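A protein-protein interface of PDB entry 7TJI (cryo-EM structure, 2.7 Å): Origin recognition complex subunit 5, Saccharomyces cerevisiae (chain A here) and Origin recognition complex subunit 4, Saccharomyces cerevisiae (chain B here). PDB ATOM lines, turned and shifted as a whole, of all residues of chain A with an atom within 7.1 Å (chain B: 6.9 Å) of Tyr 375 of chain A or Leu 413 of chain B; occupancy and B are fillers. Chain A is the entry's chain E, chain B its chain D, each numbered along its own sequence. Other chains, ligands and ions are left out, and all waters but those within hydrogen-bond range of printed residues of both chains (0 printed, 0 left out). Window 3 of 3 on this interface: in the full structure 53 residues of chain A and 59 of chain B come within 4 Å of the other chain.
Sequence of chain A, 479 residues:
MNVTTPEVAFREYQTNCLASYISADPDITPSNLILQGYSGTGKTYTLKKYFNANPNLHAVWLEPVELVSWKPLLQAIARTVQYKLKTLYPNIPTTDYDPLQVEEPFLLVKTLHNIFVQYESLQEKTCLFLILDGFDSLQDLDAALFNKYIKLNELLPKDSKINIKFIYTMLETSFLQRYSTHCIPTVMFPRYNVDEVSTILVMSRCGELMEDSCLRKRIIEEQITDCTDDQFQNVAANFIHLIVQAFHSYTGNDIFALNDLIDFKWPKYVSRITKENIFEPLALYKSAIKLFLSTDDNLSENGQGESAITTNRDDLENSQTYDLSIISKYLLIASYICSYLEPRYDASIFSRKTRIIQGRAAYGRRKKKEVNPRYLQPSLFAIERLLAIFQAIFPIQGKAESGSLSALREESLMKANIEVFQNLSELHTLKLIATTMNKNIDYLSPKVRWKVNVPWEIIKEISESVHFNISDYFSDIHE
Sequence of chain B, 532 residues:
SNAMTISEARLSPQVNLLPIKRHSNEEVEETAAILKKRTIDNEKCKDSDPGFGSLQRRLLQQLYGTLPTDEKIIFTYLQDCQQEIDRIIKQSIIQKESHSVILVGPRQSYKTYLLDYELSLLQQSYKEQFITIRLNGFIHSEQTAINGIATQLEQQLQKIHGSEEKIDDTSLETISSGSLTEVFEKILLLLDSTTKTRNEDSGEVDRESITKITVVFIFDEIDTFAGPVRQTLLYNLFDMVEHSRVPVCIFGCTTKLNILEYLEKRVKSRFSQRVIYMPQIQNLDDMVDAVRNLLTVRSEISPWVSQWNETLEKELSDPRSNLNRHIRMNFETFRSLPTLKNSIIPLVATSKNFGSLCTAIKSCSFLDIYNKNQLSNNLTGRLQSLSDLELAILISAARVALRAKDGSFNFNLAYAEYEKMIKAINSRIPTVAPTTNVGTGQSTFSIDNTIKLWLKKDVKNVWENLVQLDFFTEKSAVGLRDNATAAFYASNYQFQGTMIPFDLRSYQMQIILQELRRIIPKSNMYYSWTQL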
ATOM      1  N   TYR A 336       4.661  18.012  -5.893  1.00  0.00           N
ATOM      2  CA  TYR A 336       3.338  17.462  -6.180  1.00  0.00           C
ATOM      3  C   TYR A 336       3.310  15.947  -5.988  1.00  0.00           C
ATOM      4  O   TYR A 336       2.343  15.399  -5.434  1.00  0.00           O
ATOM      5  CB  TYR A 336       2.918  17.825  -7.604  1.00  0.00           C
ATOM      6  CG  TYR A 336       1.429  17.769  -7.832  1.00  0.00           C
ATOM      7  CD1 TYR A 336       0.622  18.864  -7.550  1.00  0.00           C
ATOM      8  CD2 TYR A 336       0.823  16.610  -8.307  1.00  0.00           C
ATOM      9  CE1 TYR A 336      -0.739  18.816  -7.750  1.00  0.00           C
ATOM     10  CE2 TYR A 336      -0.540  16.548  -8.509  1.00  0.00           C
ATOM     11  CZ  TYR A 336      -1.315  17.652  -8.225  1.00  0.00           C
ATOM     12  OH  TYR A 336      -2.672  17.597  -8.421  1.00  0.00           O
ATOM     13  N   TYR A 340       1.044  14.054  -3.109  1.00  0.00           N
ATOM     14  CA  TYR A 340      -0.099  13.257  -3.540  1.00  0.00           C
ATOM     15  C   TYR A 340       0.197  11.769  -3.672  1.00  0.00           C
ATOM     16  O   TYR A 340      -0.673  11.020  -4.123  1.00  0.00           O
ATOM     17  CB  TYR A 340      -0.655  13.816  -4.846  1.00  0.00           C
ATOM     18  CG  TYR A 340      -1.427  15.083  -4.599  1.00  0.00           C
ATOM     19  CD1 TYR A 340      -2.677  15.042  -3.998  1.00  0.00           C
ATOM     20  CD2 TYR A 340      -0.888  16.322  -4.912  1.00  0.00           C
ATOM     21  CE1 TYR A 340      -3.382  16.194  -3.746  1.00  0.00           C
ATOM     22  CE2 TYR A 340      -1.589  17.481  -4.659  1.00  0.00           C
ATOM     23  CZ  TYR A 340      -2.835  17.410  -4.077  1.00  0.00           C
ATOM     24  OH  TYR A 340      -3.540  18.562  -3.828  1.00  0.00           O
ATOM     25  N   VAL A 371     -10.351   6.897  -4.760  1.00  0.00           N
ATOM     26  CA  VAL A 371     -10.644   8.159  -4.088  1.00  0.00           C
ATOM     27  C   VAL A 371     -10.212   9.376  -4.888  1.00  0.00           C
ATOM     28  O   VAL A 371     -10.756  10.473  -4.648  1.00  0.00           O
ATOM     29  CB  VAL A 371     -10.020   8.182  -2.668  1.00  0.00           C
ATOM     30  CG1 VAL A 371      -8.580   8.701  -2.673  1.00  0.00           C
ATOM     31  CG2 VAL A 371     -10.897   8.978  -1.705  1.00  0.00           C
ATOM     32  N   ASN A 372      -9.303   9.225  -5.881  1.00  0.00           N
ATOM     33  CA  ASN A 372      -8.684  10.285  -6.676  1.00  0.00           C
ATOM     34  C   ASN A 372      -8.085  11.342  -5.757  1.00  0.00           C
ATOM     35  O   ASN A 372      -8.712  12.387  -5.531  1.00  0.00           O
ATOM     36  CB  ASN A 372      -9.675  10.908  -7.663  1.00  0.00           C
ATOM     37  CG  ASN A 372      -8.988  11.605  -8.829  1.00  0.00           C
ATOM     38  OD1 ASN A 372      -8.092  12.428  -8.646  1.00  0.00           O
ATOM     39  ND2 ASN A 372      -9.419  11.279 -10.042  1.00  0.00           N
ATOM     40  N   PRO A 373      -6.904  11.080  -5.179  1.00  0.00           N
ATOM     41  CA  PRO A 373      -6.373  11.936  -4.098  1.00  0.00           C
ATOM     42  C   PRO A 373      -6.091  13.381  -4.489  1.00  0.00           C
ATOM     43  O   PRO A 373      -5.953  14.224  -3.596  1.00  0.00           O
ATOM     44  CB  PRO A 373      -5.080  11.220  -3.692  1.00  0.00           C
ATOM     45  CG  PRO A 373      -4.673  10.472  -4.910  1.00  0.00           C
ATOM     46  CD  PRO A 373      -5.940  10.042  -5.585  1.00  0.00           C
ATOM     47  N   ARG A 374      -6.031  13.698  -5.778  1.00  0.00           N
ATOM     48  CA  ARG A 374      -5.870  15.069  -6.236  1.00  0.00           C
ATOM     49  C   ARG A 374      -7.135  15.908  -6.075  1.00  0.00           C
ATOM     50  O   ARG A 374      -7.084  17.118  -6.314  1.00  0.00           O
ATOM     51  CB  ARG A 374      -5.403  15.063  -7.692  1.00  0.00           C
ATOM     52  CG  ARG A 374      -4.211  14.134  -7.921  1.00  0.00           C
ATOM     53  CD  ARG A 374      -3.865  13.990  -9.392  1.00  0.00           C
ATOM     54  NE  ARG A 374      -4.309  12.716  -9.941  1.00  0.00           N
ATOM     55  CZ  ARG A 374      -5.055  12.585 -11.030  1.00  0.00           C
ATOM     56  NH1 ARG A 374      -5.464  13.638 -11.718  1.00  0.00           N
ATOM     57  NH2 ARG A 374      -5.398  11.368 -11.438  1.00  0.00           N
ATOM     58  N   TYR A 375      -8.259  15.306  -5.688  1.00  0.00           N
ATOM     59  CA  TYR A 375      -9.442  16.048  -5.275  1.00  0.00           C
ATOM     60  C   TYR A 375      -9.328  16.639  -3.875  1.00  0.00           C
ATOM     61  O   TYR A 375     -10.023  17.614  -3.581  1.00  0.00           O
ATOM     62  CB  TYR A 375     -10.690  15.158  -5.314  1.00  0.00           C
ATOM     63  CG  TYR A 375     -11.195  14.822  -6.692  1.00  0.00           C
ATOM     64  CD1 TYR A 375     -11.038  15.708  -7.750  1.00  0.00           C
ATOM     65  CD2 TYR A 375     -11.855  13.626  -6.931  1.00  0.00           C
ATOM     66  CE1 TYR A 375     -11.511  15.398  -9.015  1.00  0.00           C
ATOM     67  CE2 TYR A 375     -12.323  13.308  -8.187  1.00  0.00           C
ATOM     68  CZ  TYR A 375     -12.151  14.199  -9.223  1.00  0.00           C
ATOM     69  OH  TYR A 375     -12.624  13.881 -10.472  1.00  0.00           O
ATOM     70  N   LEU A 376      -8.498  16.071  -3.008  1.00  0.00           N
ATOM     71  CA  LEU A 376      -8.397  16.502  -1.621  1.00  0.00           C
ATOM     72  C   LEU A 376      -7.128  17.321  -1.397  1.00  0.00           C
ATOM     73  O   LEU A 376      -6.323  17.539  -2.306  1.00  0.00           O
ATOM     74  CB  LEU A 376      -8.457  15.309  -0.660  1.00  0.00           C
ATOM     75  CG  LEU A 376      -9.480  14.182  -0.850  1.00  0.00           C
ATOM     76  CD1 LEU A 376      -8.953  13.022  -1.675  1.00  0.00           C
ATOM     77  CD2 LEU A 376      -9.981  13.693   0.503  1.00  0.00           C
ATOM     78  N   GLN A 377      -6.976  17.786  -0.158  1.00  0.00           N
ATOM     79  CA  GLN A 377      -5.870  18.654   0.214  1.00  0.00           C
ATOM     80  C   GLN A 377      -4.557  17.866   0.275  1.00  0.00           C
ATOM     81  O   GLN A 377      -4.555  16.675   0.597  1.00  0.00           O
ATOM     82  CB  GLN A 377      -6.162  19.313   1.563  1.00  0.00           C
ATOM     83  CG  GLN A 377      -7.135  20.476   1.471  1.00  0.00           C
ATOM     84  CD  GLN A 377      -7.308  21.205   2.791  1.00  0.00           C
ATOM     85  OE1 GLN A 377      -6.516  21.033   3.718  1.00  0.00           O
ATOM     86  NE2 GLN A 377      -8.350  22.023   2.883  1.00  0.00           N
ATOM     87  N   SER B 396     -25.791  18.808  -6.248  1.00  0.00           N
ATOM     88  CA  SER B 396     -24.578  17.990  -6.290  1.00  0.00           C
ATOM     89  C   SER B 396     -23.752  18.126  -5.014  1.00  0.00           C
ATOM     90  O   SER B 396     -23.260  17.125  -4.472  1.00  0.00           O
ATOM     91  CB  SER B 396     -23.735  18.374  -7.504  1.00  0.00           C
ATOM     92  OG  SER B 396     -24.524  18.418  -8.676  1.00  0.00           O
ATOM     93  N   ALA B 397     -23.616  19.356  -4.506  1.00  0.00           N
ATOM     94  CA  ALA B 397     -22.884  19.578  -3.262  1.00  0.00           C
ATOM     95  C   ALA B 397     -23.598  18.955  -2.070  1.00  0.00           C
ATOM     96  O   ALA B 397     -22.947  18.430  -1.158  1.00  0.00           O
ATOM     97  CB  ALA B 397     -22.671  21.072  -3.035  1.00  0.00           C
ATOM     98  N   VAL B 400     -22.802  15.213  -2.197  1.00  0.00           N
ATOM     99  CA  VAL B 400     -21.446  14.933  -1.722  1.00  0.00           C
ATOM    100  C   VAL B 400     -21.354  15.110  -0.209  1.00  0.00           C
ATOM    101  O   VAL B 400     -20.704  14.317   0.482  1.00  0.00           O
ATOM    102  CB  VAL B 400     -20.429  15.815  -2.475  1.00  0.00           C
ATOM    103  CG1 VAL B 400     -19.011  15.609  -1.951  1.00  0.00           C
ATOM    104  CG2 VAL B 400     -20.471  15.505  -3.954  1.00  0.00           C
ATOM    105  N   ARG B 403     -23.021  12.090   1.514  1.00  0.00           N
ATOM    106  CA  ARG B 403     -22.208  10.875   1.500  1.00  0.00           C
ATOM    107  C   ARG B 403     -20.982  10.982   2.400  1.00  0.00           C
ATOM    108  O   ARG B 403     -20.494   9.963   2.900  1.00  0.00           O
ATOM    109  CB  ARG B 403     -21.791  10.531   0.075  1.00  0.00           C
ATOM    110  CG  ARG B 403     -22.749   9.591  -0.614  1.00  0.00           C
ATOM    111  CD  ARG B 403     -22.178   9.128  -1.923  1.00  0.00           C
ATOM    112  NE  ARG B 403     -21.575  10.239  -2.645  1.00  0.00           N
ATOM    113  CZ  ARG B 403     -22.134  10.840  -3.683  1.00  0.00           C
ATOM    114  NH1 ARG B 403     -23.304  10.449  -4.161  1.00  0.00           N
ATOM    115  NH2 ARG B 403     -21.508  11.862  -4.254  1.00  0.00           N
ATOM    116  N   SER B 408     -18.542  17.420   4.783  1.00  0.00           N
ATOM    117  CA  SER B 408     -17.670  18.396   4.158  1.00  0.00           C
ATOM    118  C   SER B 408     -17.390  18.021   2.710  1.00  0.00           C
ATOM    119  O   SER B 408     -17.386  16.844   2.341  1.00  0.00           O
ATOM    120  CB  SER B 408     -16.357  18.530   4.930  1.00  0.00           C
ATOM    121  OG  SER B 408     -15.631  19.663   4.498  1.00  0.00           O
ATOM    122  N   PHE B 409     -17.155  19.047   1.898  1.00  0.00           N
ATOM    123  CA  PHE B 409     -17.019  18.904   0.457  1.00  0.00           C
ATOM    124  C   PHE B 409     -16.185  20.067  -0.056  1.00  0.00           C
ATOM    125  O   PHE B 409     -15.920  21.031   0.663  1.00  0.00           O
ATOM    126  CB  PHE B 409     -18.391  18.855  -0.238  1.00  0.00           C
ATOM    127  CG  PHE B 409     -19.251  20.069   0.003  1.00  0.00           C
ATOM    128  CD1 PHE B 409     -20.069  20.143   1.119  1.00  0.00           C
ATOM    129  CD2 PHE B 409     -19.267  21.126  -0.898  1.00  0.00           C
ATOM    130  CE1 PHE B 409     -20.850  21.253   1.348  1.00  0.00           C
ATOM    131  CE2 PHE B 409     -20.058  22.239  -0.668  1.00  0.00           C
ATOM    132  CZ  PHE B 409     -20.850  22.296   0.452  1.00  0.00           C
ATOM    133  N   ASN B 410     -15.776  19.970  -1.317  1.00  0.00           N
ATOM    134  CA  ASN B 410     -15.098  21.066  -1.989  1.00  0.00           C
ATOM    135  C   ASN B 410     -15.671  21.214  -3.391  1.00  0.00           C
ATOM    136  O   ASN B 410     -16.623  20.530  -3.774  1.00  0.00           O
ATOM    137  CB  ASN B 410     -13.575  20.859  -2.017  1.00  0.00           C
ATOM    138  CG  ASN B 410     -13.174  19.458  -2.439  1.00  0.00           C
ATOM    139  OD1 ASN B 410     -13.516  18.995  -3.524  1.00  0.00           O
ATOM    140  ND2 ASN B 410     -12.435  18.779  -1.575  1.00  0.00           N
ATOM    141  N   PHE B 411     -15.071  22.125  -4.156  1.00  0.00           N
ATOM    142  CA  PHE B 411     -15.538  22.425  -5.505  1.00  0.00           C
ATOM    143  C   PHE B 411     -15.288  21.267  -6.466  1.00  0.00           C
ATOM    144  O   PHE B 411     -16.097  21.033  -7.372  1.00  0.00           O
ATOM    145  CB  PHE B 411     -14.853  23.705  -5.990  1.00  0.00           C
ATOM    146  CG  PHE B 411     -15.224  24.116  -7.380  1.00  0.00           C
ATOM    147  CD1 PHE B 411     -16.395  24.811  -7.613  1.00  0.00           C
ATOM    148  CD2 PHE B 411     -14.385  23.839  -8.452  1.00  0.00           C
ATOM    149  CE1 PHE B 411     -16.734  25.204  -8.885  1.00  0.00           C
ATOM    150  CE2 PHE B 411     -14.724  24.223  -9.728  1.00  0.00           C
ATOM    151  CZ  PHE B 411     -15.898  24.908  -9.946  1.00  0.00           C
ATOM    152  N   ASN B 412     -14.180  20.540  -6.286  1.00  0.00           N
ATOM    153  CA  ASN B 412     -13.821  19.458  -7.200  1.00  0.00           C
ATOM    154  C   ASN B 412     -14.793  18.289  -7.102  1.00  0.00           C
ATOM    155  O   ASN B 412     -15.241  17.758  -8.127  1.00  0.00           O
ATOM    156  CB  ASN B 412     -12.396  18.984  -6.917  1.00  0.00           C
ATOM    157  CG  ASN B 412     -11.354  19.997  -7.320  1.00  0.00           C
ATOM    158  OD1 ASN B 412     -11.572  20.801  -8.221  1.00  0.00           O
ATOM    159  ND2 ASN B 412     -10.212  19.963  -6.653  1.00  0.00           N
ATOM    160  N   LEU B 413     -15.143  17.885  -5.880  1.00  0.00           N
ATOM    161  CA  LEU B 413     -16.050  16.758  -5.695  1.00  0.00           C
ATOM    162  C   LEU B 413     -17.469  17.114  -6.122  1.00  0.00           C
ATOM    163  O   LEU B 413     -18.183  16.279  -6.695  1.00  0.00           O
ATOM    164  CB  LEU B 413     -16.012  16.303  -4.237  1.00  0.00           C
ATOM    165  CG  LEU B 413     -14.647  15.798  -3.768  1.00  0.00           C
ATOM    166  CD1 LEU B 413     -14.503  15.927  -2.265  1.00  0.00           C
ATOM    167  CD2 LEU B 413     -14.435  14.365  -4.201  1.00  0.00           C
ATOM    168  N   ALA B 414     -17.882  18.356  -5.867  1.00  0.00           N
ATOM    169  CA  ALA B 414     -19.192  18.817  -6.310  1.00  0.00           C
ATOM    170  C   ALA B 414     -19.267  18.897  -7.828  1.00  0.00           C
ATOM    171  O   ALA B 414     -20.300  18.561  -8.417  1.00  0.00           O
ATOM    172  CB  ALA B 414     -19.514  20.167  -5.677  1.00  0.00           C
ATOM    173  N   TYR B 415     -18.175  19.304  -8.484  1.00  0.00           N
ATOM    174  CA  TYR B 415     -18.170  19.297  -9.943  1.00  0.00           C
ATOM    175  C   TYR B 415     -18.167  17.883 -10.507  1.00  0.00           C
ATOM    176  O   TYR B 415     -18.756  17.648 -11.568  1.00  0.00           O
ATOM    177  CB  TYR B 415     -16.981  20.077 -10.496  1.00  0.00           C
ATOM    178  CG  TYR B 415     -17.095  20.300 -11.986  1.00  0.00           C
ATOM    179  CD1 TYR B 415     -17.898  21.314 -12.488  1.00  0.00           C
ATOM    180  CD2 TYR B 415     -16.430  19.474 -12.893  1.00  0.00           C
ATOM    181  CE1 TYR B 415     -18.023  21.514 -13.842  1.00  0.00           C
ATOM    182  CE2 TYR B 415     -16.550  19.668 -14.248  1.00  0.00           C
ATOM    183  CZ  TYR B 415     -17.346  20.692 -14.717  1.00  0.00           C
ATOM    184  OH  TYR B 415     -17.472  20.893 -16.067  1.00  0.00           O
ATOM    185  N   ALA B 416     -17.494  16.943  -9.833  1.00  0.00           N
ATOM    186  CA  ALA B 416     -17.529  15.548 -10.270  1.00  0.00           C
ATOM    187  C   ALA B 416     -18.941  14.977 -10.186  1.00  0.00           C
ATOM    188  O   ALA B 416     -19.416  14.331 -11.131  1.00  0.00           O
ATOM    189  CB  ALA B 416     -16.556  14.714  -9.440  1.00  0.00           C
ATOM    190  N   GLU B 417     -19.638  15.250  -9.075  1.00  0.00           N
ATOM    191  CA  GLU B 417     -21.030  14.827  -8.930  1.00  0.00           C
ATOM    192  C   GLU B 417     -21.930  15.498  -9.961  1.00  0.00           C
ATOM    193  O   GLU B 417     -22.842  14.862 -10.506  1.00  0.00           O
ATOM    194  CB  GLU B 417     -21.517  15.126  -7.512  1.00  0.00           C
ATOM    195  CG  GLU B 417     -22.953  14.717  -7.224  1.00  0.00           C
ATOM    196  CD  GLU B 417     -23.137  13.219  -7.181  1.00  0.00           C
ATOM    197  OE1 GLU B 417     -22.704  12.597  -6.195  1.00  0.00           O
ATOM    198  OE2 GLU B 417     -23.721  12.659  -8.133  1.00  0.00           O
ATOM    199  N   TYR B 418     -21.669  16.773 -10.261  1.00  0.00           N
ATOM    200  CA  TYR B 418     -22.471  17.502 -11.238  1.00  0.00           C
ATOM    201  C   TYR B 418     -22.307  16.936 -12.643  1.00  0.00           C
ATOM    202  O   TYR B 418     -23.295  16.760 -13.366  1.00  0.00           O
ATOM    203  CB  TYR B 418     -22.088  18.976 -11.219  1.00  0.00           C
ATOM    204  CG  TYR B 418     -22.622  19.754 -12.390  1.00  0.00           C
ATOM    205  CD1 TYR B 418     -23.975  20.041 -12.492  1.00  0.00           C
ATOM    206  CD2 TYR B 418     -21.770  20.217 -13.388  1.00  0.00           C
ATOM    207  CE1 TYR B 418     -24.467  20.764 -13.553  1.00  0.00           C
ATOM    208  CE2 TYR B 418     -22.256  20.933 -14.455  1.00  0.00           C
ATOM    209  CZ  TYR B 418     -23.605  21.199 -14.536  1.00  0.00           C
ATOM    210  OH  TYR B 418     -24.084  21.915 -15.606  1.00  0.00           O
ATOM    211  N   GLU B 419     -21.063  16.656 -13.049  1.00  0.00           N
ATOM    212  CA  GLU B 419     -20.837  16.114 -14.383  1.00  0.00           C
ATOM    213  C   GLU B 419     -21.369  14.688 -14.491  1.00  0.00           C
ATOM    214  O   GLU B 419     -21.902  14.315 -15.544  1.00  0.00           O
ATOM    215  CB  GLU B 419     -19.347  16.218 -14.759  1.00  0.00           C
ATOM    216  CG  GLU B 419     -18.483  14.960 -14.622  1.00  0.00           C
ATOM    217  CD  GLU B 419     -16.992  15.263 -14.629  1.00  0.00           C
ATOM    218  OE1 GLU B 419     -16.397  15.305 -15.726  1.00  0.00           O
ATOM    219  OE2 GLU B 419     -16.413  15.457 -13.538  1.00  0.00           O
ATOM    220  N   LYS B 420     -21.315  13.918 -13.394  1.00  0.00           N
ATOM    221  CA  LYS B 420     -21.912  12.587 -13.376  1.00  0.00           C
ATOM    222  C   LYS B 420     -23.427  12.655 -13.531  1.00  0.00           C
ATOM    223  O   LYS B 420     -24.019  11.875 -14.290  1.00  0.00           O
ATOM    224  CB  LYS B 420     -21.523  11.888 -12.075  1.00  0.00           C
ATOM    225  CG  LYS B 420     -21.959  10.457 -11.943  1.00  0.00           C
ATOM    226  CD  LYS B 420     -21.190   9.774 -10.827  1.00  0.00           C
ATOM    227  CE  LYS B 420     -19.691   9.791 -11.092  1.00  0.00           C
ATOM    228  NZ  LYS B 420     -18.908  10.340  -9.951  1.00  0.00           N
ATOM    229  N   LYS B 456     -15.605  23.946 -15.524  1.00  0.00           N
ATOM    230  CA  LYS B 456     -15.251  24.354 -14.164  1.00  0.00           C
ATOM    231  C   LYS B 456     -15.009  25.856 -14.069  1.00  0.00           C
ATOM    232  O   LYS B 456     -15.322  26.481 -13.044  1.00  0.00           O
ATOM    233  CB  LYS B 456     -14.008  23.593 -13.703  1.00  0.00           C
ATOM    234  CG  LYS B 456     -14.298  22.315 -12.944  1.00  0.00           C
ATOM    235  CD  LYS B 456     -13.042  21.508 -12.706  1.00  0.00           C
ATOM    236  CE  LYS B 456     -13.208  20.536 -11.550  1.00  0.00           C
ATOM    237  NZ  LYS B 456     -12.845  21.127 -10.237  1.00  0.00           N
ATOM    238  N   ASP B 503     -10.554  25.551  -5.013  1.00  0.00           N
ATOM    239  CA  ASP B 503     -11.141  24.256  -5.328  1.00  0.00           C
ATOM    240  C   ASP B 503     -10.885  23.213  -4.250  1.00  0.00           C
ATOM    241  O   ASP B 503     -11.451  22.119  -4.327  1.00  0.00           O
ATOM    242  CB  ASP B 503     -10.615  23.748  -6.673  1.00  0.00           C
ATOM    243  CG  ASP B 503      -9.103  23.741  -6.741  1.00  0.00           C
ATOM    244  OD1 ASP B 503      -8.506  24.824  -6.925  1.00  0.00           O
ATOM    245  OD2 ASP B 503      -8.512  22.648  -6.610  1.00  0.00           O
ATOM    246  N   LEU B 504     -10.051  23.521  -3.257  1.00  0.00           N
ATOM    247  CA  LEU B 504      -9.758  22.609  -2.166  1.00  0.00           C
ATOM    248  C   LEU B 504     -10.297  23.082  -0.821  1.00  0.00           C
ATOM    249  O   LEU B 504     -10.079  22.400   0.184  1.00  0.00           O
ATOM    250  CB  LEU B 504      -8.243  22.387  -2.056  1.00  0.00           C
ATOM    251  CG  LEU B 504      -7.555  21.700  -3.236  1.00  0.00           C
ATOM    252  CD1 LEU B 504      -6.087  21.445  -2.925  1.00  0.00           C
ATOM    253  CD2 LEU B 504      -8.262  20.411  -3.596  1.00  0.00           C
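O of Tyr 375 of chain A is in hydrogen-bond range of ND2 of Asn 410 of chain B. The backbone carbonyl oxygen (O) of Leu 504 of chain B lies within hydrogen-bond range of the side-chain amide nitrogen (NE2) of Gln 377 of chain A (3.2 Å).
The side-chain amide oxygen (OD1) of Asn 410 of chain B sits at hydrogen-bond distance from the backbone NH (N) of Asn 412 of chain B (3.2 Å). The side-chain amide oxygen of Asn 412 of chain B sits at hydrogen-bond distance from the side-chain amino group of Lys 456 of chain B (2.4 Å). The side-chain amide oxygen (OD1) of Asn 410 of chain B lies within hydrogen-bond range of the backbone NH (N) of Leu 413 of chain B, at 3.1 Å. OH of Tyr 340 of chain A is in hydrogen-bond range of O of Leu 376 of chain A (3.3 Å). The side-chain amide nitrogen (ND2) of Asn 412 of chain B sits at hydrogen-bond distance from the side-chain carboxylate (OD2) of Asp 503 of chain B (3.2 Å).
Tyr 340 of chain A touches Leu 504 of chain B (OH to CD1, 3.95 Å). Tyr 375 of chain A touches Asn 412 of chain B. Tyr 375 of chain A touches Leu 413 of chain B (CD2 to CD2, 3.8 Å). Tyr 375 of chain A touches Leu 504 of chain B (O to CD2, 3.3 Å). CD2 of Leu 504 of chain B touches O of Leu 376 of chain A, at 3.7 Å.
Tyr 375 of chain A touches just these residues of chain B: Asn 410 (3.3 Å), Asn 412 (3.6 Å), Leu 413 (3.8 Å) and Leu 504 (3.3 Å). Leu 413 of chain B touches just one residue of chain A: Tyr 375. Printed residues of chain B within 4 Å of Gln 377 of chain A: Leu 504. Printed residues of chain A within 4 Å of Asn 412 of chain B: Tyr 375. Of the printed residues of chain A, Leu 504 of chain B touches Tyr 340, Tyr 375, Leu 376 and Gln 377. The nearest residue of chain B that does not touch Tyr 375 of chain A is Ala 416 of chain B (4.1 Å).
Printed residues of chain A that touch a printed residue of chain B: Tyr 340, Tyr 375, Leu 376 and Gln 377. Hydrophobic or aromatic side chains of chain A that line the printed part of chain B: Tyr 340 and Tyr 375. Of the 20 printed residues of chain B, 4 touch a printed residue of chain A. Printed residues of chain B that touch a printed residue of chain A: Asn 410, Asn 412, Leu 413 and Leu 504. Along chain B the printed residues that touch a printed residue of chain A span positions 410 to 504. Among the printed residues, 7 pairs touch across the chains.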
